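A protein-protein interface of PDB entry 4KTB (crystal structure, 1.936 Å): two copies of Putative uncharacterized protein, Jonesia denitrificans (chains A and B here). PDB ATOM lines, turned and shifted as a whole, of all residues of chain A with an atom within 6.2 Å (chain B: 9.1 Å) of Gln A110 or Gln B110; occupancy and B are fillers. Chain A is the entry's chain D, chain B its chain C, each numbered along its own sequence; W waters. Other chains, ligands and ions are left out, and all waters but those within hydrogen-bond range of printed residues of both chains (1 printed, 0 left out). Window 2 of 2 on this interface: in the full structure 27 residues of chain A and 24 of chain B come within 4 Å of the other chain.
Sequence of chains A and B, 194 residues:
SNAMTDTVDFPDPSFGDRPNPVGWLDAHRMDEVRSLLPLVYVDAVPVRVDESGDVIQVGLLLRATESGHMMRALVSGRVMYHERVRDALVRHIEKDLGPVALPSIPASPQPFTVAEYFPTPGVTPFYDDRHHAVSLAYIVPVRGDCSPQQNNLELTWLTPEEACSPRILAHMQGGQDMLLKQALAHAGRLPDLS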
ATOM      1  N   PRO A 106     -35.644  -1.997  31.089  1.00  0.00           N
ATOM      2  CA  PRO A 106     -35.858  -2.110  29.647  1.00  0.00           C
ATOM      3  C   PRO A 106     -34.756  -2.930  29.032  1.00  0.00           C
ATOM      4  O   PRO A 106     -33.597  -2.780  29.424  1.00  0.00           O
ATOM      5  CB  PRO A 106     -35.739  -0.663  29.152  1.00  0.00           C
ATOM      6  CG  PRO A 106     -35.931   0.186  30.355  1.00  0.00           C
ATOM      7  CD  PRO A 106     -35.368  -0.607  31.491  1.00  0.00           C
ATOM      8  N   SER A 108     -33.758  -2.642  26.005  1.00  0.00           N
ATOM      9  CA  SER A 108     -32.963  -1.732  25.198  1.00  0.00           C
ATOM     10  C   SER A 108     -32.252  -0.723  26.054  1.00  0.00           C
ATOM     11  O   SER A 108     -32.852  -0.135  26.953  1.00  0.00           O
ATOM     12  CB  SER A 108     -33.852  -0.952  24.253  1.00  0.00           C
ATOM     13  OG  SER A 108     -33.064  -0.040  23.512  1.00  0.00           O
ATOM     14  N   PRO A 109     -30.967  -0.509  25.764  1.00  0.00           N
ATOM     15  CA  PRO A 109     -30.250   0.589  26.406  1.00  0.00           C
ATOM     16  C   PRO A 109     -30.663   1.967  25.895  1.00  0.00           C
ATOM     17  O   PRO A 109     -30.118   2.933  26.407  1.00  0.00           O
ATOM     18  CB  PRO A 109     -28.780   0.308  26.065  1.00  0.00           C
ATOM     19  CG  PRO A 109     -28.818  -0.650  24.901  1.00  0.00           C
ATOM     20  CD  PRO A 109     -30.064  -1.448  25.076  1.00  0.00           C
ATOM     21  N   GLN A 110     -31.584   2.077  24.934  1.00  0.00           N
ATOM     22  CA  GLN A 110     -32.024   3.407  24.495  1.00  0.00           C
ATOM     23  C   GLN A 110     -32.914   4.052  25.558  1.00  0.00           C
ATOM     24  O   GLN A 110     -34.034   3.592  25.789  1.00  0.00           O
ATOM     25  CB  GLN A 110     -32.792   3.351  23.166  1.00  0.00           C
ATOM     26  CG  GLN A 110     -33.152   4.735  22.583  1.00  0.00           C
ATOM     27  CD  GLN A 110     -34.059   4.662  21.362  1.00  0.00           C
ATOM     28  OE1 GLN A 110     -35.045   3.918  21.345  1.00  0.00           O
ATOM     29  NE2 GLN A 110     -33.740   5.449  20.335  1.00  0.00           N
ATOM     30  N   PRO A 111     -32.423   5.125  26.205  1.00  0.00           N
ATOM     31  CA  PRO A 111     -33.234   5.819  27.213  1.00  0.00           C
ATOM     32  C   PRO A 111     -34.314   6.662  26.561  1.00  0.00           C
ATOM     33  O   PRO A 111     -34.206   6.980  25.374  1.00  0.00           O
ATOM     34  CB  PRO A 111     -32.224   6.735  27.903  1.00  0.00           C
ATOM     35  CG  PRO A 111     -31.238   7.065  26.808  1.00  0.00           C
ATOM     36  CD  PRO A 111     -31.122   5.785  25.997  1.00  0.00           C
ATOM     37  N   PHE A 112     -35.342   7.038  27.310  1.00  0.00           N
ATOM     38  CA  PHE A 112     -36.364   7.883  26.707  1.00  0.00           C
ATOM     39  C   PHE A 112     -35.839   9.299  26.470  1.00  0.00           C
ATOM     40  O   PHE A 112     -36.319  10.005  25.586  1.00  0.00           O
ATOM     41  CB  PHE A 112     -37.693   7.855  27.478  1.00  0.00           C
ATOM     42  CG  PHE A 112     -37.700   8.675  28.736  1.00  0.00           C
ATOM     43  CD1 PHE A 112     -37.936  10.041  28.692  1.00  0.00           C
ATOM     44  CD2 PHE A 112     -37.517   8.070  29.969  1.00  0.00           C
ATOM     45  CE1 PHE A 112     -37.952  10.795  29.854  1.00  0.00           C
ATOM     46  CE2 PHE A 112     -37.539   8.811  31.130  1.00  0.00           C
ATOM     47  CZ  PHE A 112     -37.758  10.176  31.080  1.00  0.00           C
ATOM     48  N   THR A 113     -34.841   9.702  27.248  1.00  0.00           N
ATOM     49  CA  THR A 113     -34.128  10.941  26.978  1.00  0.00           C
ATOM     50  C   THR A 113     -32.843  10.984  27.752  1.00  0.00           C
ATOM     51  O   THR A 113     -32.562  10.107  28.550  1.00  0.00           O
ATOM     52  CB  THR A 113     -34.926  12.187  27.355  1.00  0.00           C
ATOM     53  OG1 THR A 113     -34.348  13.317  26.695  1.00  0.00           O
ATOM     54  CG2 THR A 113     -34.884  12.417  28.862  1.00  0.00           C
ATOM     55  N   VAL A 114     -32.067  12.022  27.500  1.00  0.00           N
ATOM     56  CA  VAL A 114     -30.834  12.246  28.221  1.00  0.00           C
ATOM     57  C   VAL A 114     -30.896  13.585  28.957  1.00  0.00           C
ATOM     58  O   VAL A 114     -30.927  14.648  28.339  1.00  0.00           O
ATOM     59  CB  VAL A 114     -29.637  12.208  27.275  1.00  0.00           C
ATOM     60  CG1 VAL A 114     -28.371  12.619  28.010  1.00  0.00           C
ATOM     61  CG2 VAL A 114     -29.491  10.816  26.656  1.00  0.00           C
ATOM     62  N   ALA A 137     -32.196   8.595  31.212  1.00  0.00           N
ATOM     63  CA  ALA A 137     -33.529   8.488  31.792  1.00  0.00           C
ATOM     64  C   ALA A 137     -34.337   7.351  31.204  1.00  0.00           C
ATOM     65  O   ALA A 137     -34.477   7.239  29.977  1.00  0.00           O
ATOM     66  CB  ALA A 137     -34.281   9.794  31.654  1.00  0.00           C
ATOM     67  N   TYR A 138     -34.895   6.538  32.099  1.00  0.00           N
ATOM     68  CA  TYR A 138     -35.729   5.416  31.721  1.00  0.00           C
ATOM     69  C   TYR A 138     -37.027   5.371  32.498  1.00  0.00           C
ATOM     70  O   TYR A 138     -37.092   5.725  33.683  1.00  0.00           O
ATOM     71  CB  TYR A 138     -35.017   4.120  32.018  1.00  0.00           C
ATOM     72  CG  TYR A 138     -33.780   3.887  31.227  1.00  0.00           C
ATOM     73  CD1 TYR A 138     -32.551   4.307  31.700  1.00  0.00           C
ATOM     74  CD2 TYR A 138     -33.832   3.206  30.023  1.00  0.00           C
ATOM     75  CE1 TYR A 138     -31.406   4.067  30.988  1.00  0.00           C
ATOM     76  CE2 TYR A 138     -32.695   2.963  29.298  1.00  0.00           C
ATOM     77  CZ  TYR A 138     -31.482   3.398  29.787  1.00  0.00           C
ATOM     78  OH  TYR A 138     -30.332   3.166  29.075  1.00  0.00           O
ATOM     79  N   HIS A 186     -43.472  10.933  26.762  1.00  0.00           N
ATOM     80  CA  HIS A 186     -42.969   9.778  26.042  1.00  0.00           C
ATOM     81  C   HIS A 186     -43.917   8.590  26.185  1.00  0.00           C
ATOM     82  O   HIS A 186     -43.954   7.720  25.318  1.00  0.00           O
ATOM     83  CB  HIS A 186     -41.593   9.386  26.543  1.00  0.00           C
ATOM     84  CG  HIS A 186     -40.859   8.473  25.618  1.00  0.00           C
ATOM     85  ND1 HIS A 186     -40.556   7.167  25.942  1.00  0.00           N
ATOM     86  CD2 HIS A 186     -40.355   8.680  24.380  1.00  0.00           C
ATOM     87  CE1 HIS A 186     -39.902   6.606  24.941  1.00  0.00           C
ATOM     88  NE2 HIS A 186     -39.766   7.500  23.981  1.00  0.00           N
ATOM     89  N   VAL B  85     -24.042  17.705  25.472  1.00  0.00           N
ATOM     90  CA  VAL B  85     -23.804  16.585  24.584  1.00  0.00           C
ATOM     91  C   VAL B  85     -23.858  16.951  23.101  1.00  0.00           C
ATOM     92  O   VAL B  85     -22.950  16.602  22.346  1.00  0.00           O
ATOM     93  CB  VAL B  85     -24.805  15.473  24.879  1.00  0.00           C
ATOM     94  CG1 VAL B  85     -24.585  14.301  23.948  1.00  0.00           C
ATOM     95  CG2 VAL B  85     -24.667  15.040  26.328  1.00  0.00           C
ATOM     96  N   ARG B  86     -24.910  17.653  22.678  1.00  0.00           N
ATOM     97  CA  ARG B  86     -25.037  18.004  21.261  1.00  0.00           C
ATOM     98  C   ARG B  86     -23.885  18.916  20.842  1.00  0.00           C
ATOM     99  O   ARG B  86     -23.427  18.858  19.700  1.00  0.00           O
ATOM    100  CB  ARG B  86     -26.407  18.626  20.940  1.00  0.00           C
ATOM    101  CG  ARG B  86     -26.704  19.936  21.663  1.00  0.00           C
ATOM    102  CD  ARG B  86     -28.056  20.533  21.237  1.00  0.00           C
ATOM    103  NE  ARG B  86     -29.180  19.735  21.716  1.00  0.00           N
ATOM    104  CZ  ARG B  86     -29.980  19.007  20.948  1.00  0.00           C
ATOM    105  NH1 ARG B  86     -30.961  18.299  21.492  1.00  0.00           N
ATOM    106  NH2 ARG B  86     -29.801  18.989  19.642  1.00  0.00           N
ATOM    107  N   LEU B  89     -21.013  16.694  20.273  1.00  0.00           N
ATOM    108  CA  LEU B  89     -21.276  16.197  18.928  1.00  0.00           C
ATOM    109  C   LEU B  89     -20.786  17.197  17.885  1.00  0.00           C
ATOM    110  O   LEU B  89     -20.061  16.841  16.949  1.00  0.00           O
ATOM    111  CB  LEU B  89     -22.771  15.955  18.741  1.00  0.00           C
ATOM    112  CG  LEU B  89     -23.305  14.780  19.542  1.00  0.00           C
ATOM    113  CD1 LEU B  89     -24.823  14.749  19.478  1.00  0.00           C
ATOM    114  CD2 LEU B  89     -22.710  13.476  19.005  1.00  0.00           C
ATOM    115  N   PRO B 106     -28.944  15.731  15.648  1.00  0.00           N
ATOM    116  CA  PRO B 106     -30.294  15.243  15.936  1.00  0.00           C
ATOM    117  C   PRO B 106     -30.979  16.223  16.827  1.00  0.00           C
ATOM    118  O   PRO B 106     -30.392  16.664  17.818  1.00  0.00           O
ATOM    119  CB  PRO B 106     -30.049  13.956  16.719  1.00  0.00           C
ATOM    120  CG  PRO B 106     -28.745  13.459  16.217  1.00  0.00           C
ATOM    121  CD  PRO B 106     -27.926  14.700  15.919  1.00  0.00           C
ATOM    122  N   ALA B 107     -32.205  16.567  16.472  1.00  0.00           N
ATOM    123  CA  ALA B 107     -32.960  17.534  17.233  1.00  0.00           C
ATOM    124  C   ALA B 107     -33.120  17.011  18.647  1.00  0.00           C
ATOM    125  O   ALA B 107     -33.135  17.777  19.605  1.00  0.00           O
ATOM    126  CB  ALA B 107     -34.301  17.789  16.585  1.00  0.00           C
ATOM    127  N   SER B 108     -33.198  15.689  18.763  1.00  0.00           N
ATOM    128  CA  SER B 108     -33.504  15.032  20.037  1.00  0.00           C
ATOM    129  C   SER B 108     -32.286  14.419  20.718  1.00  0.00           C
ATOM    130  O   SER B 108     -31.445  13.820  20.057  1.00  0.00           O
ATOM    131  CB  SER B 108     -34.522  13.925  19.820  1.00  0.00           C
ATOM    132  OG  SER B 108     -34.518  13.046  20.932  1.00  0.00           O
ATOM    133  N   PRO B 109     -32.208  14.554  22.053  1.00  0.00           N
ATOM    134  CA  PRO B 109     -31.048  14.026  22.778  1.00  0.00           C
ATOM    135  C   PRO B 109     -30.999  12.514  22.823  1.00  0.00           C
ATOM    136  O   PRO B 109     -29.917  11.964  23.005  1.00  0.00           O
ATOM    137  CB  PRO B 109     -31.215  14.584  24.196  1.00  0.00           C
ATOM    138  CG  PRO B 109     -32.655  14.985  24.304  1.00  0.00           C
ATOM    139  CD  PRO B 109     -33.093  15.361  22.911  1.00  0.00           C
ATOM    140  N   GLN B 110     -32.142  11.856  22.666  1.00  0.00           N
ATOM    141  CA  GLN B 110     -32.191  10.400  22.698  1.00  0.00           C
ATOM    142  C   GLN B 110     -31.243   9.781  21.669  1.00  0.00           C
ATOM    143  O   GLN B 110     -31.407   9.987  20.470  1.00  0.00           O
ATOM    144  CB  GLN B 110     -33.617   9.905  22.428  1.00  0.00           C
ATOM    145  CG  GLN B 110     -33.753   8.395  22.541  1.00  0.00           C
ATOM    146  CD  GLN B 110     -35.112   7.904  22.122  1.00  0.00           C
ATOM    147  OE1 GLN B 110     -35.647   8.321  21.089  1.00  0.00           O
ATOM    148  NE2 GLN B 110     -35.681   6.989  22.911  1.00  0.00           N
ATOM    149  N   PRO B 111     -30.247   9.015  22.137  1.00  0.00           N
ATOM    150  CA  PRO B 111     -29.360   8.334  21.190  1.00  0.00           C
ATOM    151  C   PRO B 111     -30.041   7.093  20.644  1.00  0.00           C
ATOM    152  O   PRO B 111     -31.090   6.695  21.166  1.00  0.00           O
ATOM    153  CB  PRO B 111     -28.157   7.943  22.058  1.00  0.00           C
ATOM    154  CG  PRO B 111     -28.754   7.736  23.418  1.00  0.00           C
ATOM    155  CD  PRO B 111     -29.849   8.782  23.537  1.00  0.00           C
ATOM    156  N   PHE B 112     -29.467   6.476  19.616  1.00  0.00           N
ATOM    157  CA  PHE B 112     -30.075   5.257  19.115  1.00  0.00           C
ATOM    158  C   PHE B 112     -29.702   4.093  20.007  1.00  0.00           C
ATOM    159  O   PHE B 112     -30.445   3.112  20.117  1.00  0.00           O
ATOM    160  CB  PHE B 112     -29.742   4.986  17.646  1.00  0.00           C
ATOM    161  CG  PHE B 112     -28.301   4.649  17.380  1.00  0.00           C
ATOM    162  CD1 PHE B 112     -27.859   3.340  17.432  1.00  0.00           C
ATOM    163  CD2 PHE B 112     -27.403   5.645  17.030  1.00  0.00           C
ATOM    164  CE1 PHE B 112     -26.530   3.039  17.165  1.00  0.00           C
ATOM    165  CE2 PHE B 112     -26.087   5.355  16.770  1.00  0.00           C
ATOM    166  CZ  PHE B 112     -25.646   4.047  16.832  1.00  0.00           C
ATOM    167  N   THR B 113     -28.557   4.207  20.666  1.00  0.00           N
ATOM    168  CA  THR B 113     -28.215   3.240  21.687  1.00  0.00           C
ATOM    169  C   THR B 113     -27.243   3.860  22.645  1.00  0.00           C
ATOM    170  O   THR B 113     -26.945   5.048  22.576  1.00  0.00           O
ATOM    171  CB  THR B 113     -27.585   1.962  21.104  1.00  0.00           C
ATOM    172  OG1 THR B 113     -27.426   0.988  22.141  1.00  0.00           O
ATOM    173  CG2 THR B 113     -26.236   2.265  20.528  1.00  0.00           C
ATOM    174  N   VAL B 114     -26.779   3.045  23.568  1.00  0.00           N
ATOM    175  CA  VAL B 114     -25.730   3.452  24.462  1.00  0.00           C
ATOM    176  C   VAL B 114     -24.707   2.348  24.404  1.00  0.00           C
ATOM    177  O   VAL B 114     -25.027   1.177  24.572  1.00  0.00           O
ATOM    178  CB  VAL B 114     -26.236   3.610  25.876  1.00  0.00           C
ATOM    179  CG1 VAL B 114     -25.067   3.901  26.818  1.00  0.00           C
ATOM    180  CG2 VAL B 114     -27.267   4.718  25.937  1.00  0.00           C
ATOM    181  N   ALA B 115     -23.474   2.723  24.114  1.00  0.00           N
ATOM    182  CA  ALA B 115     -22.418   1.740  24.007  1.00  0.00           C
ATOM    183  C   ALA B 115     -21.596   1.837  25.281  1.00  0.00           C
ATOM    184  O   ALA B 115     -21.080   2.907  25.616  1.00  0.00           O
ATOM    185  CB  ALA B 115     -21.564   1.998  22.790  1.00  0.00           C
ATOM    186  N   GLU B 116     -21.479   0.735  26.004  1.00  0.00           N
ATOM    187  CA  GLU B 116     -20.719   0.780  27.235  1.00  0.00           C
ATOM    188  C   GLU B 116     -19.370   0.106  27.039  1.00  0.00           C
ATOM    189  O   GLU B 116     -19.260  -1.120  27.069  1.00  0.00           O
ATOM    190  CB  GLU B 116     -21.557   0.202  28.381  1.00  0.00           C
ATOM    191  CG  GLU B 116     -22.907   0.926  28.494  1.00  0.00           C
ATOM    192  CD  GLU B 116     -23.912   0.255  29.412  1.00  0.00           C
ATOM    193  OE1 GLU B 116     -25.094   0.117  29.014  1.00  0.00           O
ATOM    194  OE2 GLU B 116     -23.538  -0.116  30.538  1.00  0.00           O
ATOM    195  N   SER B 135     -21.146   5.738  26.267  1.00  0.00           N
ATOM    196  CA  SER B 135     -21.291   6.664  25.137  1.00  0.00           C
ATOM    197  C   SER B 135     -22.719   6.766  24.617  1.00  0.00           C
ATOM    198  O   SER B 135     -23.411   5.758  24.455  1.00  0.00           O
ATOM    199  CB  SER B 135     -20.345   6.281  23.994  1.00  0.00           C
ATOM    200  OG  SER B 135     -20.181   7.356  23.093  1.00  0.00           O
ATOM    201  N   LEU B 136     -23.166   7.991  24.368  1.00  0.00           N
ATOM    202  CA  LEU B 136     -24.451   8.190  23.721  1.00  0.00           C
ATOM    203  C   LEU B 136     -24.156   8.169  22.245  1.00  0.00           C
ATOM    204  O   LEU B 136     -23.359   8.971  21.762  1.00  0.00           O
ATOM    205  CB  LEU B 136     -25.047   9.540  24.099  1.00  0.00           C
ATOM    206  CG  LEU B 136     -25.384   9.730  25.570  1.00  0.00           C
ATOM    207  CD1 LEU B 136     -25.850  11.163  25.809  1.00  0.00           C
ATOM    208  CD2 LEU B 136     -26.444   8.747  26.020  1.00  0.00           C
ATOM    209  N   ALA B 137     -24.783   7.251  21.526  1.00  0.00           N
ATOM    210  CA  ALA B 137     -24.428   7.036  20.131  1.00  0.00           C
ATOM    211  C   ALA B 137     -25.498   7.594  19.220  1.00  0.00           C
ATOM    212  O   ALA B 137     -26.686   7.337  19.413  1.00  0.00           O
ATOM    213  CB  ALA B 137     -24.178   5.556  19.838  1.00  0.00           C
ATOM    214  N   TYR B 138     -25.060   8.350  18.219  1.00  0.00           N
ATOM    215  CA  TYR B 138     -25.971   8.969  17.289  1.00  0.00           C
ATOM    216  C   TYR B 138     -25.544   8.740  15.858  1.00  0.00           C
ATOM    217  O   TYR B 138     -24.361   8.588  15.549  1.00  0.00           O
ATOM    218  CB  TYR B 138     -26.037  10.465  17.536  1.00  0.00           C
ATOM    219  CG  TYR B 138     -26.422  10.855  18.929  1.00  0.00           C
ATOM    220  CD1 TYR B 138     -25.481  10.878  19.945  1.00  0.00           C
ATOM    221  CD2 TYR B 138     -27.726  11.237  19.222  1.00  0.00           C
ATOM    222  CE1 TYR B 138     -25.829  11.259  21.227  1.00  0.00           C
ATOM    223  CE2 TYR B 138     -28.091  11.615  20.507  1.00  0.00           C
ATOM    224  CZ  TYR B 138     -27.136  11.627  21.501  1.00  0.00           C
ATOM    225  OH  TYR B 138     -27.500  12.000  22.774  1.00  0.00           O
ATOM    226  N   ILE B 139     -26.547   8.709  14.993  1.00  0.00           N
ATOM    227  CA  ILE B 139     -26.345   8.751  13.563  1.00  0.00           C
ATOM    228  C   ILE B 139     -26.429  10.213  13.161  1.00  0.00           C
ATOM    229  O   ILE B 139     -27.423  10.898  13.436  1.00  0.00           O
ATOM    230  CB  ILE B 139     -27.440   7.954  12.860  1.00  0.00           C
ATOM    231  CG1 ILE B 139     -27.226   6.463  13.113  1.00  0.00           C
ATOM    232  CG2 ILE B 139     -27.471   8.257  11.377  1.00  0.00           C
ATOM    233  CD1 ILE B 139     -28.386   5.573  12.681  1.00  0.00           C
ATOM    234  N   GLN B 182     -25.358  -1.776  14.766  1.00  0.00           N
ATOM    235  CA  GLN B 182     -26.557  -1.306  15.460  1.00  0.00           C
ATOM    236  C   GLN B 182     -27.055   0.004  14.882  1.00  0.00           C
ATOM    237  O   GLN B 182     -28.256   0.295  14.890  1.00  0.00           O
ATOM    238  CB  GLN B 182     -26.268  -1.117  16.944  1.00  0.00           C
ATOM    239  CG  GLN B 182     -25.827  -2.384  17.648  1.00  0.00           C
ATOM    240  CD  GLN B 182     -25.231  -2.092  19.005  1.00  0.00           C
ATOM    241  OE1 GLN B 182     -24.072  -2.422  19.281  1.00  0.00           O
ATOM    242  NE2 GLN B 182     -26.021  -1.454  19.860  1.00  0.00           N
ATOM    243  N   HIS B 186     -30.565   0.399  13.091  1.00  0.00           N
ATOM    244  CA  HIS B 186     -31.464   1.446  13.551  1.00  0.00           C
ATOM    245  C   HIS B 186     -32.011   2.292  12.398  1.00  0.00           C
ATOM    246  O   HIS B 186     -33.153   2.755  12.444  1.00  0.00           O
ATOM    247  CB  HIS B 186     -30.775   2.358  14.559  1.00  0.00           C
ATOM    248  CG  HIS B 186     -31.649   3.456  15.071  1.00  0.00           C
ATOM    249  ND1 HIS B 186     -32.767   3.211  15.858  1.00  0.00           N
ATOM    250  CD2 HIS B 186     -31.592   4.797  14.931  1.00  0.00           C
ATOM    251  CE1 HIS B 186     -33.339   4.350  16.167  1.00  0.00           C
ATOM    252  NE2 HIS B 186     -32.651   5.339  15.619  1.00  0.00           N
HETATM  253  O   HOH W   1     -36.504   4.732  25.135  1.00  0.00           O
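Among the printed residues, pairs that only touch across the chains: Pro A109 with Thr B113 (3.5 Å), Pro A109 with Val B114 (3.4 Å), Gln A110 with Gln B110 (3.2 Å), Gln A110 with Phe B112 (3.9 Å), Pro A111 with Pro B111 (3.9 Å), Phe A112 with Gln B110 (3.96 Å), Thr A113 with Pro B109 (3.4 Å), Val A114 with Pro B109 (3.9 Å), Val A114 with Pro B111 (3.7 Å) and Val A114 with Leu B136 (3.6 Å).
Gln A110 touches its own counterpart, Gln B110. Gln A110 touches Phe B112, and with the chains exchanged Phe A112 touches Gln B110. Pro A111 touches its own counterpart, Pro B111. Val A114 touches Pro B111, but with the chains exchanged Pro A111 does not touch Val B114 (4.0004 Å). Positions printed for both chains: 106, 108, 109, 110, 111, 112, 113, 114, 137, 138 and 186.
The backbone NH of Phe B112 is in hydrogen-bond range of the backbone carbonyl oxygen of Ala B137 (2.9 Å). The backbone NH (N) of Ala A137 lies within hydrogen-bond range of the backbone carbonyl oxygen (O) of Thr A113. O of Pro A109 sits at hydrogen-bond distance from OH of Tyr A138 (2.7 Å). The side-chain hydroxyl of Ser A108 is in hydrogen-bond range of the backbone NH of Gln A110, 2.9 Å away. The backbone NH (N) of Phe A112 sits at hydrogen-bond distance from the backbone carbonyl oxygen (O) of Ala A137 (2.8 Å). The backbone carbonyl oxygen (O) of Pro B109 lies within hydrogen-bond range of the side-chain hydroxyl (OH) of Tyr B138 (2.4 Å).
Of the 21 printed residues of chain B, 7 touch a printed residue of chain A. Hydrophobic or aromatic side chains of chain B that line the printed part of chain A: Pro B109, Pro B111, Val B114 and Leu B136. Of the 11 printed residues of chain A, 6 touch a printed residue of chain B. Printed residues of chain A that touch a printed residue of chain B: Pro A109, Gln A110, Pro A111, Phe A112, Thr A113 and Val A114. Hydrophobic or aromatic side chains of chain A that line the printed part of chain B: Pro A109, Pro A111 and Val A114. Among the printed residues, 12 pairs touch across the chains.
O of Pro A111 is in hydrogen-bond range of NE2 of Gln B110. The backbone carbonyl oxygen of Pro B111 sits at hydrogen-bond distance from the side-chain amide nitrogen of Gln A110, at 3.0 Å.
Pro A109 touches just these residues of chain B: Thr B113 (3.5 Å) and Val B114 (3.4 Å). Printed residues of chain B within 4 Å of Gln A110: Gln B110, Pro B111 and Phe B112. Of the printed residues of chain B, Val A114 touches Pro B109 (3.9 Å), Pro B111 (3.7 Å) and Leu B136 (3.6 Å). Arg B86 touches none of the printed residues of chain A. Printed residues of chain A within 4 Å of Pro B109: Thr A113 (3.4 Å) and Val A114 (3.9 Å). Printed residues of chain A within 4 Å of Phe B112: Gln A110. Of the printed residues of chain A, Val B114 touches Pro A109. The nearest residue of chain A that does not touch Gln B110 is His A186 (4.3 Å). The nearest printed residue of chain A that does not touch Val B114 is Pro A111 (4.0004 Å).
Water W1 lies within hydrogen-bond range of O of Gln A110, O of Pro A111, NE2 of Gln B110 and N of Phe A112.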
